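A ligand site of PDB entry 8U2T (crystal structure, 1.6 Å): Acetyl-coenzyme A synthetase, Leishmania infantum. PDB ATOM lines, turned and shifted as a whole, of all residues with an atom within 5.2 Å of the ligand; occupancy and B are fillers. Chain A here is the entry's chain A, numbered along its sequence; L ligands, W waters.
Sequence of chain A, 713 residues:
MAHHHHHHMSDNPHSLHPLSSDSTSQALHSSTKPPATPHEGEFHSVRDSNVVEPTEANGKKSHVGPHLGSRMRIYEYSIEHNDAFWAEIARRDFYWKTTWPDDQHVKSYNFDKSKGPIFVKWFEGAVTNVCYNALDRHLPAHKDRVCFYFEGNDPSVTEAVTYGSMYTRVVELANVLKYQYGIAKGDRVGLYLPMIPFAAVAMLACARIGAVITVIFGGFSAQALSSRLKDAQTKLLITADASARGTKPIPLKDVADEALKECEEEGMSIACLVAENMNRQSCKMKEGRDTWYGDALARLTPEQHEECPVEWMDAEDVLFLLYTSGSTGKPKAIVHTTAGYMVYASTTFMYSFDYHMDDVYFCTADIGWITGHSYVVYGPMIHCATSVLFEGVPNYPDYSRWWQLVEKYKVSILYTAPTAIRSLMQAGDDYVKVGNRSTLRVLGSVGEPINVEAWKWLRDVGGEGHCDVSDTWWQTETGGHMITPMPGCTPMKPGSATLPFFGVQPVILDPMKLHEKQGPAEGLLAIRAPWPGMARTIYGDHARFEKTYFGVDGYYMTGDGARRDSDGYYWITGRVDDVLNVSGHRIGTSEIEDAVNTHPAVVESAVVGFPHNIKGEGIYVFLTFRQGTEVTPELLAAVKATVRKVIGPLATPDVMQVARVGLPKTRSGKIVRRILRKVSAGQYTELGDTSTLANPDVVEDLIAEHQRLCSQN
NE2 of Gln 475 is in hydrogen-bond range of O of Thr 558, at 2.8 Å.
The side-chain carboxylate of Asp 560 lies within hydrogen-bond range of the indole nitrogen of Trp 473 (3.0 Å).
NE2 of Gln 475 sits close to NH1 of Arg 575 (3.5 Å).
O of Ser 445 is in hydrogen-bond range of N of Thr 472 (3.0 Å).
The side-chain amide oxygen (OD1) of Asn 581 sits close to the backbone NH (N) of Gly 584.
The side-chain carboxylate of Glu 477 lies within salt-bridge range of the guanidinium group of Arg 586.
The backbone carbonyl oxygen (O) of Gly 447 sits at hydrogen-bond distance from the side-chain amide nitrogen (ND2) of Asn 581, 2.8 Å away.
N of Asp 560 is in hydrogen-bond range of OG1 of Thr 558, at 3.0 Å.
O of Glu 448 sits close to N4 of the ligand, 3.3 Å away.
Ile 370 touches the ligand.
N of Pro 449 touches C9 of the ligand (3.2 Å).
Trp 473 touches the ligand (CD1 to C7, 3.6 Å).
O of Trp 474 touches C6 of the ligand, at 3.4 Å.
CG2 of Ile 572 touches C9 of the ligand (3.8 Å).
Asn 581 touches the ligand (ND2 to O5, 3.7 Å).
Hydrophobic or aromatic side chains that line the ligand: Ile 370, Pro 449, Trp 473 and Ile 572.
Water W2 lies within hydrogen-bond range of the side-chain carboxylate (OD1) of Asp 471, the backbone carbonyl oxygen (O) of Glu 448, the side-chain hydroxyl (OG) of Ser 445 and a nitrogen (N3) of the ligand.
The guanidinium group of Arg 575 sits at hydrogen-bond distance from an oxygen (O6) of the ligand, at 2.9 Å.
OD1 of Asp 471 is in hydrogen-bond range of N3 of the ligand, at 2.9 Å.
NE2 of Gln 475 sits at hydrogen-bond distance from O6 of the ligand (3.0 Å).
The guanidinium group of Arg 586 is in salt-bridge range of an oxygen (O3) of the ligand (2.7 Å).
The side-chain carboxylate of Asp 560 sits at hydrogen-bond distance from an oxygen (O6) of the ligand.
An oxygen (O3) of the ligand lies within hydrogen-bond range of the backbone NH of Thr 476, 2.9 Å away.
O of Thr 472 lies within hydrogen-bond range of N3 of the ligand (2.9 Å).
N2 of the ligand lies within hydrogen-bond range of N of Gly 447.
The side-chain hydroxyl of Thr 476 sits at hydrogen-bond distance from an oxygen (O3) of the ligand, 2.7 Å away.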
ATOM      1  N   THR A 324       4.293   9.273   8.455  1.00  0.00           N
ATOM      2  CA  THR A 324       4.727   8.434   9.563  1.00  0.00           C
ATOM      3  C   THR A 324       3.710   7.325   9.747  1.00  0.00           C
ATOM      4  O   THR A 324       2.498   7.572   9.720  1.00  0.00           O
ATOM      5  CB  THR A 324       4.831   9.266  10.859  1.00  0.00           C
ATOM      6  OG1 THR A 324       5.692  10.404  10.632  1.00  0.00           O
ATOM      7  CG2 THR A 324       5.348   8.426  12.006  1.00  0.00           C
ATOM      8  N   ILE A 370      12.524  11.762  10.791  1.00  0.00           N
ATOM      9  CA  ILE A 370      12.587  12.947  11.639  1.00  0.00           C
ATOM     10  C   ILE A 370      14.017  13.193  12.143  1.00  0.00           C
ATOM     11  O   ILE A 370      14.425  14.342  12.327  1.00  0.00           O
ATOM     12  CB  ILE A 370      11.568  12.828  12.790  1.00  0.00           C
ATOM     13  CG1 ILE A 370      11.454  14.146  13.559  1.00  0.00           C
ATOM     14  CG2 ILE A 370      11.910  11.699  13.705  1.00  0.00           C
ATOM     15  CD1 ILE A 370      10.728  15.272  12.763  1.00  0.00           C
ATOM     16  N   SER A 445      22.547   7.631  20.578  1.00  0.00           N
ATOM     17  CA  SER A 445      21.779   6.522  20.034  1.00  0.00           C
ATOM     18  C   SER A 445      20.340   6.962  19.886  1.00  0.00           C
ATOM     19  O   SER A 445      19.793   7.601  20.803  1.00  0.00           O
ATOM     20  CB  SER A 445      21.888   5.292  20.950  1.00  0.00           C
ATOM     21  OG  SER A 445      21.229   4.203  20.375  1.00  0.00           O
ATOM     22  N   VAL A 446      19.729   6.614  18.764  1.00  0.00           N
ATOM     23  CA  VAL A 446      18.331   6.994  18.549  1.00  0.00           C
ATOM     24  C   VAL A 446      17.542   5.884  17.875  1.00  0.00           C
ATOM     25  O   VAL A 446      18.067   5.162  17.018  1.00  0.00           O
ATOM     26  CB  VAL A 446      18.248   8.264  17.714  1.00  0.00           C
ATOM     27  CG1 VAL A 446      18.982   8.071  16.398  1.00  0.00           C
ATOM     28  CG2 VAL A 446      16.785   8.626  17.527  1.00  0.00           C
ATOM     29  N   GLY A 447      16.280   5.757  18.263  1.00  0.00           N
ATOM     30  CA  GLY A 447      15.257   5.125  17.441  1.00  0.00           C
ATOM     31  C   GLY A 447      14.759   3.795  17.935  1.00  0.00           C
ATOM     32  O   GLY A 447      13.738   3.315  17.407  1.00  0.00           O
ATOM     33  N   GLU A 448      15.409   3.194  18.919  1.00  0.00           N
ATOM     34  CA  GLU A 448      15.036   1.868  19.390  1.00  0.00           C
ATOM     35  C   GLU A 448      15.738   1.619  20.713  1.00  0.00           C
ATOM     36  O   GLU A 448      16.702   2.313  21.054  1.00  0.00           O
ATOM     37  CB  GLU A 448      15.408   0.788  18.354  1.00  0.00           C
ATOM     38  CG  GLU A 448      16.867   0.866  17.924  1.00  0.00           C
ATOM     39  CD  GLU A 448      17.146   0.200  16.568  1.00  0.00           C
ATOM     40  OE1 GLU A 448      16.721  -0.957  16.415  1.00  0.00           O
ATOM     41  OE2 GLU A 448      17.801   0.843  15.689  1.00  0.00           O
ATOM     42  N   PRO A 449      15.283   0.638  21.475  1.00  0.00           N
ATOM     43  CA  PRO A 449      16.011   0.250  22.686  1.00  0.00           C
ATOM     44  C   PRO A 449      17.417  -0.225  22.336  1.00  0.00           C
ATOM     45  O   PRO A 449      17.680  -0.763  21.261  1.00  0.00           O
ATOM     46  CB  PRO A 449      15.172  -0.890  23.256  1.00  0.00           C
ATOM     47  CG  PRO A 449      13.835  -0.758  22.619  1.00  0.00           C
ATOM     48  CD  PRO A 449      14.080  -0.189  21.277  1.00  0.00           C
ATOM     49  N   ASP A 471      21.622   8.254  24.930  1.00  0.00           N
ATOM     50  CA  ASP A 471      20.482   7.471  24.434  1.00  0.00           C
ATOM     51  C   ASP A 471      19.252   8.367  24.519  1.00  0.00           C
ATOM     52  O   ASP A 471      18.717   8.584  25.623  1.00  0.00           O
ATOM     53  CB  ASP A 471      20.345   6.194  25.272  1.00  0.00           C
ATOM     54  CG  ASP A 471      19.180   5.324  24.849  1.00  0.00           C
ATOM     55  OD1 ASP A 471      18.535   5.650  23.812  1.00  0.00           O
ATOM     56  OD2 ASP A 471      18.906   4.325  25.581  1.00  0.00           O
ATOM     57  N   THR A 472      18.782   8.881  23.368  1.00  0.00           N
ATOM     58  CA  THR A 472      17.751   9.903  23.320  1.00  0.00           C
ATOM     59  C   THR A 472      16.432   9.246  22.973  1.00  0.00           C
ATOM     60  O   THR A 472      16.318   8.690  21.876  1.00  0.00           O
ATOM     61  CB  THR A 472      18.048  10.951  22.241  1.00  0.00           C
ATOM     62  OG1 THR A 472      18.161  10.305  20.959  1.00  0.00           O
ATOM     63  CG2 THR A 472      19.354  11.680  22.492  1.00  0.00           C
ATOM     64  N   TRP A 473      15.422   9.375  23.835  1.00  0.00           N
ATOM     65  CA  TRP A 473      14.089   8.911  23.506  1.00  0.00           C
ATOM     66  C   TRP A 473      13.284  10.093  23.042  1.00  0.00           C
ATOM     67  O   TRP A 473      13.313  11.146  23.678  1.00  0.00           O
ATOM     68  CB  TRP A 473      13.366   8.221  24.696  1.00  0.00           C
ATOM     69  CG  TRP A 473      11.999   7.895  24.253  1.00  0.00           C
ATOM     70  CD1 TRP A 473      11.607   6.784  23.579  1.00  0.00           C
ATOM     71  CD2 TRP A 473      10.851   8.739  24.339  1.00  0.00           C
ATOM     72  NE1 TRP A 473      10.265   6.867  23.279  1.00  0.00           N
ATOM     73  CE2 TRP A 473       9.780   8.061  23.726  1.00  0.00           C
ATOM     74  CE3 TRP A 473      10.614   9.987  24.904  1.00  0.00           C
ATOM     75  CZ2 TRP A 473       8.493   8.598  23.638  1.00  0.00           C
ATOM     76  CZ3 TRP A 473       9.327  10.524  24.815  1.00  0.00           C
ATOM     77  CH2 TRP A 473       8.297   9.837  24.174  1.00  0.00           C
ATOM     78  N   TRP A 474      12.596   9.929  21.909  1.00  0.00           N
ATOM     79  CA  TRP A 474      11.689  10.910  21.316  1.00  0.00           C
ATOM     80  C   TRP A 474      10.981  10.237  20.126  1.00  0.00           C
ATOM     81  O   TRP A 474      11.161   9.050  19.870  1.00  0.00           O
ATOM     82  CB  TRP A 474      12.455  12.167  20.914  1.00  0.00           C
ATOM     83  CG  TRP A 474      13.503  11.954  19.844  1.00  0.00           C
ATOM     84  CD1 TRP A 474      14.619  11.133  19.918  1.00  0.00           C
ATOM     85  CD2 TRP A 474      13.544  12.582  18.554  1.00  0.00           C
ATOM     86  NE1 TRP A 474      15.343  11.228  18.743  1.00  0.00           N
ATOM     87  CE2 TRP A 474      14.701  12.094  17.890  1.00  0.00           C
ATOM     88  CE3 TRP A 474      12.731  13.509  17.901  1.00  0.00           C
ATOM     89  CZ2 TRP A 474      15.047  12.481  16.597  1.00  0.00           C
ATOM     90  CZ3 TRP A 474      13.086  13.911  16.623  1.00  0.00           C
ATOM     91  CH2 TRP A 474      14.234  13.383  15.983  1.00  0.00           C
ATOM     92  N   GLN A 475      10.152  11.001  19.425  1.00  0.00           N
ATOM     93  CA  GLN A 475       9.372  10.490  18.311  1.00  0.00           C
ATOM     94  C   GLN A 475       9.166  11.591  17.273  1.00  0.00           C
ATOM     95  O   GLN A 475       9.333  12.777  17.560  1.00  0.00           O
ATOM     96  CB  GLN A 475       7.989   9.975  18.728  1.00  0.00           C
ATOM     97  CG  GLN A 475       7.813   9.663  20.185  1.00  0.00           C
ATOM     98  CD  GLN A 475       6.381   9.317  20.502  1.00  0.00           C
ATOM     99  OE1 GLN A 475       5.593  10.172  20.871  1.00  0.00           O
ATOM    100  NE2 GLN A 475       6.057   8.039  20.379  1.00  0.00           N
ATOM    101  N   THR A 476       8.751  11.164  16.068  1.00  0.00           N
ATOM    102  CA  THR A 476       8.396  12.144  15.034  1.00  0.00           C
ATOM    103  C   THR A 476       7.486  13.240  15.589  1.00  0.00           C
ATOM    104  O   THR A 476       7.713  14.442  15.361  1.00  0.00           O
ATOM    105  CB  THR A 476       7.739  11.446  13.852  1.00  0.00           C
ATOM    106  OG1 THR A 476       8.623  10.471  13.311  1.00  0.00           O
ATOM    107  CG2 THR A 476       7.410  12.437  12.744  1.00  0.00           C
ATOM    108  N   GLU A 477       6.482  12.846  16.360  1.00  0.00           N
ATOM    109  CA  GLU A 477       5.483  13.759  16.901  1.00  0.00           C
ATOM    110  C   GLU A 477       6.029  14.712  17.962  1.00  0.00           C
ATOM    111  O   GLU A 477       5.330  15.684  18.286  1.00  0.00           O
ATOM    112  CB  GLU A 477       4.335  12.946  17.508  1.00  0.00           C
ATOM    113  CG  GLU A 477       3.617  12.025  16.491  1.00  0.00           C
ATOM    114  CD  GLU A 477       4.157  10.591  16.477  1.00  0.00           C
ATOM    115  OE1 GLU A 477       5.357  10.380  16.735  1.00  0.00           O
ATOM    116  OE2 GLU A 477       3.371   9.674  16.157  1.00  0.00           O
ATOM    117  N   THR A 558       2.195   8.772  24.255  1.00  0.00           N
ATOM    118  CA  THR A 558       3.261   8.475  23.311  1.00  0.00           C
ATOM    119  C   THR A 558       3.030   7.215  22.475  1.00  0.00           C
ATOM    120  O   THR A 558       3.586   7.114  21.368  1.00  0.00           O
ATOM    121  CB  THR A 558       4.617   8.316  24.037  1.00  0.00           C
ATOM    122  OG1 THR A 558       4.586   7.132  24.857  1.00  0.00           O
ATOM    123  CG2 THR A 558       4.921   9.531  24.894  1.00  0.00           C
ATOM    124  N   ASP A 560       4.232   4.437  23.671  1.00  0.00           N
ATOM    125  CA  ASP A 560       5.262   3.600  24.275  1.00  0.00           C
ATOM    126  C   ASP A 560       4.928   3.229  25.723  1.00  0.00           C
ATOM    127  O   ASP A 560       4.259   3.981  26.440  1.00  0.00           O
ATOM    128  CB  ASP A 560       6.610   4.311  24.287  1.00  0.00           C
ATOM    129  CG  ASP A 560       7.213   4.420  22.912  1.00  0.00           C
ATOM    130  OD1 ASP A 560       7.223   3.414  22.187  1.00  0.00           O
ATOM    131  OD2 ASP A 560       7.675   5.527  22.568  1.00  0.00           O
ATOM    132  N   ILE A 572      12.549   2.826  28.450  1.00  0.00           N
ATOM    133  CA  ILE A 572      11.483   2.679  27.466  1.00  0.00           C
ATOM    134  C   ILE A 572      11.461   1.223  27.029  1.00  0.00           C
ATOM    135  O   ILE A 572      12.487   0.649  26.671  1.00  0.00           O
ATOM    136  CB  ILE A 572      11.669   3.639  26.282  1.00  0.00           C
ATOM    137  CG1 ILE A 572      11.321   5.066  26.726  1.00  0.00           C
ATOM    138  CG2 ILE A 572      10.673   3.292  25.180  1.00  0.00           C
ATOM    139  CD1 ILE A 572      12.374   5.766  27.463  1.00  0.00           C
ATOM    140  N   GLY A 574       9.124  -0.186  24.695  1.00  0.00           N
ATOM    141  CA  GLY A 574       8.676  -0.419  23.341  1.00  0.00           C
ATOM    142  C   GLY A 574       7.242   0.029  23.143  1.00  0.00           C
ATOM    143  O   GLY A 574       6.541   0.435  24.074  1.00  0.00           O
ATOM    144  N   ARG A 575       6.796  -0.078  21.891  1.00  0.00           N
ATOM    145  CA  ARG A 575       5.440   0.324  21.532  1.00  0.00           C
ATOM    146  C   ARG A 575       4.428  -0.632  22.149  1.00  0.00           C
ATOM    147  O   ARG A 575       4.632  -1.846  22.183  1.00  0.00           O
ATOM    148  CB  ARG A 575       5.232   0.317  20.018  1.00  0.00           C
ATOM    149  CG  ARG A 575       6.228   1.148  19.220  1.00  0.00           C
ATOM    150  CD  ARG A 575       6.008   2.652  19.356  1.00  0.00           C
ATOM    151  NE  ARG A 575       4.669   3.094  18.969  1.00  0.00           N
ATOM    152  CZ  ARG A 575       4.374   4.336  18.595  1.00  0.00           C
ATOM    153  NH1 ARG A 575       5.317   5.250  18.422  1.00  0.00           N
ATOM    154  NH2 ARG A 575       3.102   4.658  18.374  1.00  0.00           N
ATOM    155  N   ASN A 581       8.960  -1.764  14.870  1.00  0.00           N
ATOM    156  CA  ASN A 581      10.176  -0.974  14.836  1.00  0.00           C
ATOM    157  C   ASN A 581      11.233  -1.845  14.179  1.00  0.00           C
ATOM    158  O   ASN A 581      11.881  -2.670  14.831  1.00  0.00           O
ATOM    159  CB  ASN A 581      10.590  -0.535  16.214  1.00  0.00           C
ATOM    160  CG  ASN A 581      11.657   0.532  16.170  1.00  0.00           C
ATOM    161  OD1 ASN A 581      12.401   0.639  15.182  1.00  0.00           O
ATOM    162  ND2 ASN A 581      11.745   1.327  17.227  1.00  0.00           N
ATOM    163  N   GLY A 584      14.957   0.523  13.340  1.00  0.00           N
ATOM    164  CA  GLY A 584      14.725   1.921  13.647  1.00  0.00           C
ATOM    165  C   GLY A 584      13.559   2.565  12.912  1.00  0.00           C
ATOM    166  O   GLY A 584      13.140   3.660  13.294  1.00  0.00           O
ATOM    167  N   ARG A 586       9.662   2.847  11.821  1.00  0.00           N
ATOM    168  CA  ARG A 586       8.346   2.411  12.251  1.00  0.00           C
ATOM    169  C   ARG A 586       7.477   2.152  11.013  1.00  0.00           C
ATOM    170  O   ARG A 586       7.489   2.917  10.041  1.00  0.00           O
ATOM    171  CB  ARG A 586       7.749   3.414  13.244  1.00  0.00           C
ATOM    172  CG  ARG A 586       6.923   4.512  12.725  1.00  0.00           C
ATOM    173  CD  ARG A 586       6.955   5.697  13.733  1.00  0.00           C
ATOM    174  NE  ARG A 586       5.642   5.864  14.328  1.00  0.00           N
ATOM    175  CZ  ARG A 586       5.245   6.920  15.034  1.00  0.00           C
ATOM    176  NH1 ARG A 586       6.105   7.822  15.493  1.00  0.00           N
ATOM    177  NH2 ARG A 586       3.949   7.085  15.272  1.00  0.00           N
HETATM  178  P1  LIG L   1      10.068   7.716  15.060  1.00  0.00           P
HETATM  179  O1  LIG L   1      10.463   7.109  13.740  1.00  0.00           O
HETATM  180  O2  LIG L   1      11.197   8.529  15.654  1.00  0.00           O
HETATM  181  O3  LIG L   1       8.742   8.435  15.062  1.00  0.00           O
HETATM  182  O4  LIG L   1       9.900   6.480  16.040  1.00  0.00           O
HETATM  183  C1  LIG L   1       9.647   6.717  17.416  1.00  0.00           C
HETATM  184  C2  LIG L   1       9.552   5.435  18.188  1.00  0.00           C
HETATM  185  O5  LIG L   1      10.846   4.764  18.191  1.00  0.00           O
HETATM  186  C3  LIG L   1       9.215   5.602  19.656  1.00  0.00           C
HETATM  187  O6  LIG L   1       7.825   5.704  19.855  1.00  0.00           O
HETATM  188  C4  LIG L   1       9.805   4.362  20.285  1.00  0.00           C
HETATM  189  O7  LIG L   1       8.971   3.229  20.076  1.00  0.00           O
HETATM  190  C5  LIG L   1      11.068   4.197  19.454  1.00  0.00           C
HETATM  191  N1  LIG L   1      12.217   4.882  20.060  1.00  0.00           N
HETATM  192  C6  LIG L   1      12.771   6.020  19.637  1.00  0.00           C
HETATM  193  N2  LIG L   1      13.844   6.338  20.422  1.00  0.00           N
HETATM  194  C7  LIG L   1      13.965   5.340  21.322  1.00  0.00           C
HETATM  195  C8  LIG L   1      14.862   5.021  22.426  1.00  0.00           C
HETATM  196  N3  LIG L   1      15.867   5.888  22.663  1.00  0.00           N
HETATM  197  N4  LIG L   1      14.671   3.912  23.139  1.00  0.00           N
HETATM  198  C9  LIG L   1      13.658   3.071  22.869  1.00  0.00           C
HETATM  199  N5  LIG L   1      12.786   3.283  21.862  1.00  0.00           N
HETATM  200  C10 LIG L   1      12.902   4.378  21.084  1.00  0.00           C
HETATM  201  O   HOH W   1       9.040   7.178  11.346  1.00  0.00           O
HETATM  202  O   HOH W   2      18.633   4.191  21.535  1.00  0.00           O
HETATM  203  O   HOH W   3      10.775   1.317  21.576  1.00  0.00           O
